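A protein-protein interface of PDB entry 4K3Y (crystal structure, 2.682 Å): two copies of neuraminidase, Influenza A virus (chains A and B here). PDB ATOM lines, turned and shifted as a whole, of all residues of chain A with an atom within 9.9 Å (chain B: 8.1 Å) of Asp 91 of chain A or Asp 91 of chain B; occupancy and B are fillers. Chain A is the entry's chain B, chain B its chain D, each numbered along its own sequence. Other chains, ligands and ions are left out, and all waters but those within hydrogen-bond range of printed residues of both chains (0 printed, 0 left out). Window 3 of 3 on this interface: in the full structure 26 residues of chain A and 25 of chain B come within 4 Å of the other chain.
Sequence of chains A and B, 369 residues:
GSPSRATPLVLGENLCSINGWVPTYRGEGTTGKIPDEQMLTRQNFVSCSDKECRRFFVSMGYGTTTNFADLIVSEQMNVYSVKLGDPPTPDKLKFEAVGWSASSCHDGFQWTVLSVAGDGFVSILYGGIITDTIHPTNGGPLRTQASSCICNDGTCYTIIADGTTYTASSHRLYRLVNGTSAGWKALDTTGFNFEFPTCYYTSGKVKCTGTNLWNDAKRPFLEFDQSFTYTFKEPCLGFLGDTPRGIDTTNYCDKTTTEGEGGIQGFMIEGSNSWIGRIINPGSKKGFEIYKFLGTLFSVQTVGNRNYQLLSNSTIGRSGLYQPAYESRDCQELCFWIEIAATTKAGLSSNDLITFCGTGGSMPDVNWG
The side-chain carboxylate of Asp 91 of chain A is in salt-bridge range of the side-chain amino group of Lys 92 of chain A, at 3.7 Å.
Printed residues of chain B within 4 Å of Pro 87 of chain A: Pro 90 (3.2 Å) and Leu 93 (3.6 Å).
Pro 88 of chain B touches none of the printed residues of chain A.
Of chain A, only Glu 37 and Pro 87 come within 4 Å of Pro 90 of chain B.
No residue of chain A comes within 4 Å of Lys 92 of chain B.
Of the printed residues of chain A, Lys 94 of chain B touches Lys 83 (3.8 Å) and Gly 85 (3.6 Å).
Among the printed residues, merely in contact across the chains: Glu 37 of chain A with Pro 90 of chain B (3.6 Å), Lys 83 of chain A with Lys 94 of chain B (3.8 Å), Gly 85 of chain A with Leu 93 of chain B (3.98 Å), Gly 85 of chain A with Lys 94 of chain B (3.6 Å), Pro 87 of chain A with Pro 90 of chain B (3.2 Å), Pro 87 of chain A with Leu 93 of chain B (3.6 Å) and Asp 91 of chain A with Asp 91 of chain B (3.7 Å).
The side-chain hydroxyl (OG1) of Thr 89 of chain A is in hydrogen-bond range of the side-chain carboxylate (OD1) of Asp 91 of chain B, 3.1 Å away.
NZ of Lys 92 of chain A sits at hydrogen-bond distance from O of Asp 91 of chain B (3.4 Å).
Printed residues of chain A that touch a printed residue of chain B: Glu 37, Lys 83, Gly 85, Pro 87, Thr 89, Asp 91 and Lys 92.
Among the printed residues, no Asp or Glu carboxylate lies within 4 Å of a Lys or Arg side-chain nitrogen of the other chain.
Glu 37 of chain A touches Pro 90 of chain B, but with the chains exchanged Pro 90 of chain A does not touch Glu 37 of chain B (13.5 Å).
Thr 89 of chain A touches Asp 91 of chain B, but with the chains exchanged Asp 91 of chain A does not touch Thr 89 of chain B (9.0 Å).
Asp 91 of chain B touches its own counterpart, Asp 91 of chain A.
Lys 92 of chain A touches Asp 91 of chain B, but with the chains exchanged Asp 91 of chain A does not touch Lys 92 of chain B (5.5 Å).
13 positions are printed for both chains.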
ATOM      1  N   GLU A  28      -6.572   4.316  23.644  1.00  0.00           N
ATOM      2  CA  GLU A  28      -6.144   4.573  25.005  1.00  0.00           C
ATOM      3  C   GLU A  28      -7.351   4.787  25.921  1.00  0.00           C
ATOM      4  O   GLU A  28      -7.279   4.530  27.124  1.00  0.00           O
ATOM      5  CB  GLU A  28      -5.189   5.780  25.037  1.00  0.00           C
ATOM      6  CG  GLU A  28      -3.929   5.592  25.904  1.00  0.00           C
ATOM      7  CD  GLU A  28      -3.309   4.196  25.791  1.00  0.00           C
ATOM      8  OE1 GLU A  28      -2.901   3.815  24.669  1.00  0.00           O
ATOM      9  OE2 GLU A  28      -3.225   3.483  26.827  1.00  0.00           O
ATOM     10  N   PRO A  35      -5.370  11.166  26.542  1.00  0.00           N
ATOM     11  CA  PRO A  35      -4.459  12.315  26.477  1.00  0.00           C
ATOM     12  C   PRO A  35      -5.121  13.482  25.754  1.00  0.00           C
ATOM     13  O   PRO A  35      -5.675  13.282  24.666  1.00  0.00           O
ATOM     14  CB  PRO A  35      -3.300  11.778  25.634  1.00  0.00           C
ATOM     15  CG  PRO A  35      -3.283  10.304  25.927  1.00  0.00           C
ATOM     16  CD  PRO A  35      -4.723   9.910  26.105  1.00  0.00           C
ATOM     17  N   ASP A  36      -5.066  14.679  26.337  1.00  0.00           N
ATOM     18  CA  ASP A  36      -5.775  15.836  25.777  1.00  0.00           C
ATOM     19  C   ASP A  36      -5.016  16.492  24.621  1.00  0.00           C
ATOM     20  O   ASP A  36      -5.529  17.406  23.963  1.00  0.00           O
ATOM     21  CB  ASP A  36      -6.091  16.863  26.867  1.00  0.00           C
ATOM     22  CG  ASP A  36      -5.887  16.310  28.261  1.00  0.00           C
ATOM     23  OD1 ASP A  36      -4.722  16.020  28.620  1.00  0.00           O
ATOM     24  OD2 ASP A  36      -6.892  16.164  28.991  1.00  0.00           O
ATOM     25  N   GLU A  37      -3.793  16.021  24.384  1.00  0.00           N
ATOM     26  CA  GLU A  37      -3.024  16.405  23.204  1.00  0.00           C
ATOM     27  C   GLU A  37      -3.798  15.969  21.965  1.00  0.00           C
ATOM     28  O   GLU A  37      -3.879  16.692  20.967  1.00  0.00           O
ATOM     29  CB  GLU A  37      -1.662  15.706  23.212  1.00  0.00           C
ATOM     30  CG  GLU A  37      -1.056  15.517  24.597  1.00  0.00           C
ATOM     31  CD  GLU A  37      -0.616  14.086  24.850  1.00  0.00           C
ATOM     32  OE1 GLU A  37      -0.729  13.256  23.921  1.00  0.00           O
ATOM     33  OE2 GLU A  37      -0.161  13.789  25.976  1.00  0.00           O
ATOM     34  N   GLN A  38      -4.366  14.771  22.066  1.00  0.00           N
ATOM     35  CA  GLN A  38      -5.164  14.169  21.013  1.00  0.00           C
ATOM     36  C   GLN A  38      -6.423  14.963  20.689  1.00  0.00           C
ATOM     37  O   GLN A  38      -7.055  15.554  21.572  1.00  0.00           O
ATOM     38  CB  GLN A  38      -5.544  12.744  21.398  1.00  0.00           C
ATOM     39  CG  GLN A  38      -4.404  11.748  21.280  1.00  0.00           C
ATOM     40  CD  GLN A  38      -4.862  10.330  21.562  1.00  0.00           C
ATOM     41  OE1 GLN A  38      -6.062  10.018  21.493  1.00  0.00           O
ATOM     42  NE2 GLN A  38      -3.911   9.459  21.885  1.00  0.00           N
ATOM     43  N   MET A  39      -6.767  14.963  19.403  1.00  0.00           N
ATOM     44  CA  MET A  39      -7.987  15.574  18.896  1.00  0.00           C
ATOM     45  C   MET A  39      -9.260  14.888  19.394  1.00  0.00           C
ATOM     46  O   MET A  39      -9.257  13.689  19.716  1.00  0.00           O
ATOM     47  CB  MET A  39      -7.990  15.498  17.376  1.00  0.00           C
ATOM     48  CG  MET A  39      -7.373  16.670  16.697  1.00  0.00           C
ATOM     49  SD  MET A  39      -8.247  17.002  15.166  1.00  0.00           S
ATOM     50  CE  MET A  39      -8.823  18.663  15.499  1.00  0.00           C
ATOM     51  N   ARG A  54      -6.430   2.988   7.645  1.00  0.00           N
ATOM     52  CA  ARG A  54      -6.485   4.329   8.195  1.00  0.00           C
ATOM     53  C   ARG A  54      -7.751   4.555   8.970  1.00  0.00           C
ATOM     54  O   ARG A  54      -8.841   4.086   8.597  1.00  0.00           O
ATOM     55  CB  ARG A  54      -6.360   5.398   7.100  1.00  0.00           C
ATOM     56  CG  ARG A  54      -5.021   5.402   6.386  1.00  0.00           C
ATOM     57  CD  ARG A  54      -4.895   6.582   5.443  1.00  0.00           C
ATOM     58  NE  ARG A  54      -4.886   7.869   6.147  1.00  0.00           N
ATOM     59  CZ  ARG A  54      -3.828   8.377   6.781  1.00  0.00           C
ATOM     60  NH1 ARG A  54      -2.676   7.693   6.827  1.00  0.00           N
ATOM     61  NH2 ARG A  54      -3.929   9.567   7.381  1.00  0.00           N
ATOM     62  N   TYR A  62      -9.752  20.535  19.772  1.00  0.00           N
ATOM     63  CA  TYR A  62      -9.050  19.779  20.810  1.00  0.00           C
ATOM     64  C   TYR A  62      -9.750  19.699  22.183  1.00  0.00           C
ATOM     65  O   TYR A  62     -10.034  20.707  22.840  1.00  0.00           O
ATOM     66  CB  TYR A  62      -7.602  20.288  20.924  1.00  0.00           C
ATOM     67  CG  TYR A  62      -6.773  20.064  19.662  1.00  0.00           C
ATOM     68  CD1 TYR A  62      -6.841  20.945  18.579  1.00  0.00           C
ATOM     69  CD2 TYR A  62      -5.927  18.960  19.557  1.00  0.00           C
ATOM     70  CE1 TYR A  62      -6.082  20.728  17.425  1.00  0.00           C
ATOM     71  CE2 TYR A  62      -5.166  18.738  18.414  1.00  0.00           C
ATOM     72  CZ  TYR A  62      -5.241  19.617  17.354  1.00  0.00           C
ATOM     73  OH  TYR A  62      -4.466  19.360  16.239  1.00  0.00           O
ATOM     74  N   SER A  81      -7.993  12.118   9.183  1.00  0.00           N
ATOM     75  CA  SER A  81      -7.598  10.732   9.167  1.00  0.00           C
ATOM     76  C   SER A  81      -6.193  10.594   9.753  1.00  0.00           C
ATOM     77  O   SER A  81      -5.411  11.537   9.724  1.00  0.00           O
ATOM     78  CB  SER A  81      -7.651  10.178   7.734  1.00  0.00           C
ATOM     79  OG  SER A  81      -6.378  10.196   7.102  1.00  0.00           O
ATOM     80  N   VAL A  82      -5.904   9.429  10.322  1.00  0.00           N
ATOM     81  CA  VAL A  82      -4.559   9.056  10.730  1.00  0.00           C
ATOM     82  C   VAL A  82      -4.411   7.601  10.331  1.00  0.00           C
ATOM     83  O   VAL A  82      -5.396   6.939  10.001  1.00  0.00           O
ATOM     84  CB  VAL A  82      -4.349   9.191  12.265  1.00  0.00           C
ATOM     85  CG1 VAL A  82      -4.289  10.649  12.679  1.00  0.00           C
ATOM     86  CG2 VAL A  82      -5.462   8.472  13.022  1.00  0.00           C
ATOM     87  N   LYS A  83      -3.184   7.104  10.341  1.00  0.00           N
ATOM     88  CA  LYS A  83      -2.943   5.687  10.116  1.00  0.00           C
ATOM     89  C   LYS A  83      -3.478   4.955  11.340  1.00  0.00           C
ATOM     90  O   LYS A  83      -3.345   5.443  12.464  1.00  0.00           O
ATOM     91  CB  LYS A  83      -1.440   5.457   9.966  1.00  0.00           C
ATOM     92  CG  LYS A  83      -0.985   4.041   9.720  1.00  0.00           C
ATOM     93  CD  LYS A  83       0.542   4.006   9.544  1.00  0.00           C
ATOM     94  CE  LYS A  83       1.056   2.563   9.524  1.00  0.00           C
ATOM     95  NZ  LYS A  83       2.514   2.435   9.831  1.00  0.00           N
ATOM     96  N   GLY A  85      -3.366   2.913  14.360  1.00  0.00           N
ATOM     97  CA  GLY A  85      -2.267   2.541  15.237  1.00  0.00           C
ATOM     98  C   GLY A  85      -1.496   3.743  15.741  1.00  0.00           C
ATOM     99  O   GLY A  85      -0.855   3.695  16.795  1.00  0.00           O
ATOM    100  N   ASP A  86      -1.554   4.825  14.968  1.00  0.00           N
ATOM    101  CA  ASP A  86      -1.035   6.122  15.396  1.00  0.00           C
ATOM    102  C   ASP A  86      -2.132   6.847  16.165  1.00  0.00           C
ATOM    103  O   ASP A  86      -3.312   6.532  15.999  1.00  0.00           O
ATOM    104  CB  ASP A  86      -0.599   6.953  14.182  1.00  0.00           C
ATOM    105  CG  ASP A  86       0.556   6.314  13.409  1.00  0.00           C
ATOM    106  OD1 ASP A  86       1.064   5.246  13.835  1.00  0.00           O
ATOM    107  OD2 ASP A  86       0.968   6.904  12.382  1.00  0.00           O
ATOM    108  N   PRO A  87      -1.750   7.790  17.038  1.00  0.00           N
ATOM    109  CA  PRO A  87      -2.768   8.583  17.736  1.00  0.00           C
ATOM    110  C   PRO A  87      -3.127   9.845  16.961  1.00  0.00           C
ATOM    111  O   PRO A  87      -2.308  10.342  16.177  1.00  0.00           O
ATOM    112  CB  PRO A  87      -2.061   8.976  19.034  1.00  0.00           C
ATOM    113  CG  PRO A  87      -0.616   9.086  18.639  1.00  0.00           C
ATOM    114  CD  PRO A  87      -0.400   7.999  17.599  1.00  0.00           C
ATOM    115  N   PRO A  88      -4.346  10.363  17.170  1.00  0.00           N
ATOM    116  CA  PRO A  88      -4.739  11.639  16.551  1.00  0.00           C
ATOM    117  C   PRO A  88      -4.098  12.892  17.183  1.00  0.00           C
ATOM    118  O   PRO A  88      -4.791  13.864  17.514  1.00  0.00           O
ATOM    119  CB  PRO A  88      -6.275  11.656  16.690  1.00  0.00           C
ATOM    120  CG  PRO A  88      -6.584  10.681  17.753  1.00  0.00           C
ATOM    121  CD  PRO A  88      -5.499   9.627  17.716  1.00  0.00           C
ATOM    122  N   THR A  89      -2.775  12.863  17.316  1.00  0.00           N
ATOM    123  CA  THR A  89      -1.983  14.047  17.644  1.00  0.00           C
ATOM    124  C   THR A  89      -1.673  14.834  16.356  1.00  0.00           C
ATOM    125  O   THR A  89      -1.524  14.241  15.280  1.00  0.00           O
ATOM    126  CB  THR A  89      -0.660  13.639  18.306  1.00  0.00           C
ATOM    127  OG1 THR A  89       0.125  12.888  17.369  1.00  0.00           O
ATOM    128  CG2 THR A  89      -0.922  12.794  19.546  1.00  0.00           C
ATOM    129  N   PRO A  90      -1.576  16.173  16.467  1.00  0.00           N
ATOM    130  CA  PRO A  90      -1.284  17.121  15.380  1.00  0.00           C
ATOM    131  C   PRO A  90      -0.243  16.638  14.353  1.00  0.00           C
ATOM    132  O   PRO A  90      -0.445  16.813  13.150  1.00  0.00           O
ATOM    133  CB  PRO A  90      -0.732  18.321  16.138  1.00  0.00           C
ATOM    134  CG  PRO A  90      -1.479  18.303  17.431  1.00  0.00           C
ATOM    135  CD  PRO A  90      -1.776  16.866  17.755  1.00  0.00           C
ATOM    136  N   ASP A  91       0.851  16.047  14.828  1.00  0.00           N
ATOM    137  CA  ASP A  91       1.923  15.563  13.955  1.00  0.00           C
ATOM    138  C   ASP A  91       1.482  14.388  13.064  1.00  0.00           C
ATOM    139  O   ASP A  91       1.924  14.267  11.912  1.00  0.00           O
ATOM    140  CB  ASP A  91       3.154  15.205  14.802  1.00  0.00           C
ATOM    141  CG  ASP A  91       4.265  14.521  13.999  1.00  0.00           C
ATOM    142  OD1 ASP A  91       4.849  15.153  13.088  1.00  0.00           O
ATOM    143  OD2 ASP A  91       4.590  13.356  14.311  1.00  0.00           O
ATOM    144  N   LYS A  92       0.600  13.537  13.593  1.00  0.00           N
ATOM    145  CA  LYS A  92       0.142  12.349  12.866  1.00  0.00           C
ATOM    146  C   LYS A  92      -1.135  12.636  12.054  1.00  0.00           C
ATOM    147  O   LYS A  92      -1.540  11.846  11.194  1.00  0.00           O
ATOM    148  CB  LYS A  92      -0.088  11.179  13.834  1.00  0.00           C
ATOM    149  CG  LYS A  92       1.143  10.726  14.626  1.00  0.00           C
ATOM    150  CD  LYS A  92       2.092   9.873  13.784  1.00  0.00           C
ATOM    151  CE  LYS A  92       3.086   9.086  14.658  1.00  0.00           C
ATOM    152  NZ  LYS A  92       4.430   9.734  14.779  1.00  0.00           N
ATOM    153  N   LEU A  93      -1.748  13.784  12.327  1.00  0.00           N
ATOM    154  CA  LEU A  93      -2.961  14.212  11.651  1.00  0.00           C
ATOM    155  C   LEU A  93      -2.829  14.386  10.145  1.00  0.00           C
ATOM    156  O   LEU A  93      -1.730  14.516   9.613  1.00  0.00           O
ATOM    157  CB  LEU A  93      -3.442  15.523  12.257  1.00  0.00           C
ATOM    158  CG  LEU A  93      -4.661  15.375  13.162  1.00  0.00           C
ATOM    159  CD1 LEU A  93      -5.721  16.374  12.760  1.00  0.00           C
ATOM    160  CD2 LEU A  93      -5.200  13.973  13.078  1.00  0.00           C
ATOM    161  N   LYS A  94      -3.977  14.381   9.472  1.00  0.00           N
ATOM    162  CA  LYS A  94      -4.085  14.613   8.028  1.00  0.00           C
ATOM    163  C   LYS A  94      -5.464  15.175   7.720  1.00  0.00           C
ATOM    164  O   LYS A  94      -6.474  14.521   7.970  1.00  0.00           O
ATOM    165  CB  LYS A  94      -3.893  13.329   7.240  1.00  0.00           C
ATOM    166  CG  LYS A  94      -4.214  13.451   5.756  1.00  0.00           C
ATOM    167  CD  LYS A  94      -3.738  12.181   5.020  1.00  0.00           C
ATOM    168  CE  LYS A  94      -4.098  12.187   3.536  1.00  0.00           C
ATOM    169  NZ  LYS A  94      -3.615  13.420   2.864  1.00  0.00           N
ATOM    170  N   PHE A  95      -5.499  16.395   7.193  1.00  0.00           N
ATOM    171  CA  PHE A  95      -6.749  17.034   6.828  1.00  0.00           C
ATOM    172  C   PHE A  95      -7.322  16.326   5.580  1.00  0.00           C
ATOM    173  O   PHE A  95      -6.573  15.954   4.662  1.00  0.00           O
ATOM    174  CB  PHE A  95      -6.484  18.508   6.557  1.00  0.00           C
ATOM    175  CG  PHE A  95      -7.704  19.285   6.189  1.00  0.00           C
ATOM    176  CD1 PHE A  95      -8.587  19.695   7.163  1.00  0.00           C
ATOM    177  CD2 PHE A  95      -7.953  19.635   4.874  1.00  0.00           C
ATOM    178  CE1 PHE A  95      -9.715  20.425   6.839  1.00  0.00           C
ATOM    179  CE2 PHE A  95      -9.074  20.356   4.544  1.00  0.00           C
ATOM    180  CZ  PHE A  95      -9.958  20.752   5.534  1.00  0.00           C
ATOM    181  N   LYS A 345      -8.394  13.166  29.852  1.00  0.00           N
ATOM    182  CA  LYS A 345      -7.814  13.411  31.183  1.00  0.00           C
ATOM    183  C   LYS A 345      -8.437  14.618  31.899  1.00  0.00           C
ATOM    184  O   LYS A 345      -8.664  14.588  33.109  1.00  0.00           O
ATOM    185  CB  LYS A 345      -6.286  13.557  31.106  1.00  0.00           C
ATOM    186  CG  LYS A 345      -5.559  12.266  30.721  1.00  0.00           C
ATOM    187  CD  LYS A 345      -4.069  12.495  30.481  1.00  0.00           C
ATOM    188  CE  LYS A 345      -3.378  11.225  29.976  1.00  0.00           C
ATOM    189  NZ  LYS A 345      -1.909  11.410  29.751  1.00  0.00           N
ATOM    190  N   GLU B  37       5.415  12.549  31.266  1.00  0.00           N
ATOM    191  CA  GLU B  37       4.578  12.448  30.067  1.00  0.00           C
ATOM    192  C   GLU B  37       4.892  11.204  29.235  1.00  0.00           C
ATOM    193  O   GLU B  37       4.164  10.874  28.299  1.00  0.00           O
ATOM    194  CB  GLU B  37       4.654  13.716  29.205  1.00  0.00           C
ATOM    195  CG  GLU B  37       5.927  13.887  28.394  1.00  0.00           C
ATOM    196  CD  GLU B  37       7.073  14.469  29.196  1.00  0.00           C
ATOM    197  OE1 GLU B  37       6.916  14.728  30.416  1.00  0.00           O
ATOM    198  OE2 GLU B  37       8.160  14.680  28.605  1.00  0.00           O
ATOM    199  N   MET B  39       5.328   7.107  28.610  1.00  0.00           N
ATOM    200  CA  MET B  39       4.653   5.895  29.045  1.00  0.00           C
ATOM    201  C   MET B  39       5.517   5.109  30.012  1.00  0.00           C
ATOM    202  O   MET B  39       6.731   5.279  30.061  1.00  0.00           O
ATOM    203  CB  MET B  39       4.274   5.006  27.855  1.00  0.00           C
ATOM    204  CG  MET B  39       2.948   5.371  27.213  1.00  0.00           C
ATOM    205  SD  MET B  39       2.074   3.954  26.521  1.00  0.00           S
ATOM    206  CE  MET B  39       0.706   3.800  27.683  1.00  0.00           C
ATOM    207  N   TYR B  62       0.652   5.740  32.388  1.00  0.00           N
ATOM    208  CA  TYR B  62       1.648   6.806  32.347  1.00  0.00           C
ATOM    209  C   TYR B  62       2.238   7.123  33.722  1.00  0.00           C
ATOM    210  O   TYR B  62       2.135   8.247  34.219  1.00  0.00           O
ATOM    211  CB  TYR B  62       1.031   8.063  31.724  1.00  0.00           C
ATOM    212  CG  TYR B  62       0.778   7.971  30.229  1.00  0.00           C
ATOM    213  CD1 TYR B  62      -0.372   7.366  29.724  1.00  0.00           C
ATOM    214  CD2 TYR B  62       1.685   8.504  29.323  1.00  0.00           C
ATOM    215  CE1 TYR B  62      -0.602   7.290  28.354  1.00  0.00           C
ATOM    216  CE2 TYR B  62       1.466   8.431  27.957  1.00  0.00           C
ATOM    217  CZ  TYR B  62       0.323   7.825  27.475  1.00  0.00           C
ATOM    218  OH  TYR B  62       0.105   7.757  26.116  1.00  0.00           O
ATOM    219  N   VAL B  82       8.412   2.199  19.394  1.00  0.00           N
ATOM    220  CA  VAL B  82       8.859   3.491  18.890  1.00  0.00           C
ATOM    221  C   VAL B  82      10.094   3.254  18.052  1.00  0.00           C
ATOM    222  O   VAL B  82      10.695   2.177  18.118  1.00  0.00           O
ATOM    223  CB  VAL B  82       9.220   4.472  20.034  1.00  0.00           C
ATOM    224  CG1 VAL B  82       7.964   4.949  20.752  1.00  0.00           C
ATOM    225  CG2 VAL B  82      10.199   3.815  21.016  1.00  0.00           C
ATOM    226  N   ASP B  86      13.710   7.728  19.494  1.00  0.00           N
ATOM    227  CA  ASP B  86      12.555   8.492  19.934  1.00  0.00           C
ATOM    228  C   ASP B  86      12.107   8.058  21.333  1.00  0.00           C
ATOM    229  O   ASP B  86      12.102   6.874  21.652  1.00  0.00           O
ATOM    230  CB  ASP B  86      11.412   8.355  18.915  1.00  0.00           C
ATOM    231  CG  ASP B  86      11.727   9.037  17.599  1.00  0.00           C
ATOM    232  OD1 ASP B  86      12.897   9.446  17.404  1.00  0.00           O
ATOM    233  OD2 ASP B  86      10.818   9.165  16.756  1.00  0.00           O
ATOM    234  N   PRO B  87      11.747   9.028  22.183  1.00  0.00           N
ATOM    235  CA  PRO B  87      11.148   8.715  23.493  1.00  0.00           C
ATOM    236  C   PRO B  87       9.725   8.181  23.355  1.00  0.00           C
ATOM    237  O   PRO B  87       9.030   8.500  22.381  1.00  0.00           O
ATOM    238  CB  PRO B  87      11.101  10.079  24.184  1.00  0.00           C
ATOM    239  CG  PRO B  87      11.051  11.088  23.017  1.00  0.00           C
ATOM    240  CD  PRO B  87      11.962  10.478  21.989  1.00  0.00           C
ATOM    241  N   PRO B  88       9.288   7.371  24.321  1.00  0.00           N
ATOM    242  CA  PRO B  88       7.900   6.891  24.290  1.00  0.00           C
ATOM    243  C   PRO B  88       6.856   7.911  24.769  1.00  0.00           C
ATOM    244  O   PRO B  88       6.044   7.601  25.649  1.00  0.00           O
ATOM    245  CB  PRO B  88       7.924   5.651  25.197  1.00  0.00           C
ATOM    246  CG  PRO B  88       9.155   5.801  26.035  1.00  0.00           C
ATOM    247  CD  PRO B  88      10.137   6.613  25.253  1.00  0.00           C
ATOM    248  N   THR B  89       6.879   9.110  24.187  1.00  0.00           N
ATOM    249  CA  THR B  89       5.754  10.040  24.291  1.00  0.00           C
ATOM    250  C   THR B  89       4.595   9.593  23.388  1.00  0.00           C
ATOM    251  O   THR B  89       4.818   9.190  22.241  1.00  0.00           O
ATOM    252  CB  THR B  89       6.155  11.478  23.907  1.00  0.00           C
ATOM    253  OG1 THR B  89       7.059  11.452  22.790  1.00  0.00           O
ATOM    254  CG2 THR B  89       6.811  12.172  25.088  1.00  0.00           C
ATOM    255  N   PRO B  90       3.355   9.666  23.913  1.00  0.00           N
ATOM    256  CA  PRO B  90       2.090   9.325  23.247  1.00  0.00           C
ATOM    257  C   PRO B  90       2.095   9.681  21.764  1.00  0.00           C
ATOM    258  O   PRO B  90       1.634   8.900  20.930  1.00  0.00           O
ATOM    259  CB  PRO B  90       1.065  10.182  23.995  1.00  0.00           C
ATOM    260  CG  PRO B  90       1.750  10.606  25.303  1.00  0.00           C
ATOM    261  CD  PRO B  90       3.131  10.018  25.322  1.00  0.00           C
ATOM    262  N   ASP B  91       2.631  10.853  21.449  1.00  0.00           N
ATOM    263  CA  ASP B  91       2.828  11.303  20.074  1.00  0.00           C
ATOM    264  C   ASP B  91       3.665  10.340  19.216  1.00  0.00           C
ATOM    265  O   ASP B  91       3.446  10.213  18.010  1.00  0.00           O
ATOM    266  CB  ASP B  91       3.500  12.674  20.114  1.00  0.00           C
ATOM    267  CG  ASP B  91       3.169  13.523  18.905  1.00  0.00           C
ATOM    268  OD1 ASP B  91       3.164  12.985  17.773  1.00  0.00           O
ATOM    269  OD2 ASP B  91       2.900  14.730  19.085  1.00  0.00           O
ATOM    270  N   LYS B  92       4.625   9.665  19.843  1.00  0.00           N
ATOM    271  CA  LYS B  92       5.615   8.867  19.108  1.00  0.00           C
ATOM    272  C   LYS B  92       5.311   7.365  19.157  1.00  0.00           C
ATOM    273  O   LYS B  92       6.060   6.549  18.601  1.00  0.00           O
ATOM    274  CB  LYS B  92       7.026   9.136  19.660  1.00  0.00           C
ATOM    275  CG  LYS B  92       7.540  10.549  19.476  1.00  0.00           C
ATOM    276  CD  LYS B  92       8.619  10.610  18.400  1.00  0.00           C
ATOM    277  CE  LYS B  92       8.853  12.054  17.934  1.00  0.00           C
ATOM    278  NZ  LYS B  92       9.420  12.125  16.543  1.00  0.00           N
ATOM    279  N   LEU B  93       4.208   7.026  19.819  1.00  0.00           N
ATOM    280  CA  LEU B  93       3.791   5.650  20.011  1.00  0.00           C
ATOM    281  C   LEU B  93       3.097   5.033  18.793  1.00  0.00           C
ATOM    282  O   LEU B  93       2.345   5.700  18.066  1.00  0.00           O
ATOM    283  CB  LEU B  93       2.835   5.579  21.201  1.00  0.00           C
ATOM    284  CG  LEU B  93       3.402   5.052  22.513  1.00  0.00           C
ATOM    285  CD1 LEU B  93       4.891   5.308  22.606  1.00  0.00           C
ATOM    286  CD2 LEU B  93       2.680   5.720  23.658  1.00  0.00           C
ATOM    287  N   LYS B  94       3.370   3.752  18.573  1.00  0.00           N
ATOM    288  CA  LYS B  94       2.595   2.939  17.645  1.00  0.00           C
ATOM    289  C   LYS B  94       2.012   1.744  18.403  1.00  0.00           C
ATOM    290  O   LYS B  94       2.758   0.931  18.968  1.00  0.00           O
ATOM    291  CB  LYS B  94       3.465   2.442  16.488  1.00  0.00           C
ATOM    292  CG  LYS B  94       2.820   1.336  15.693  1.00  0.00           C
ATOM    293  CD  LYS B  94       3.733   0.842  14.594  1.00  0.00           C
ATOM    294  CE  LYS B  94       2.929   0.036  13.580  1.00  0.00           C
ATOM    295  NZ  LYS B  94       3.675  -0.174  12.312  1.00  0.00           N
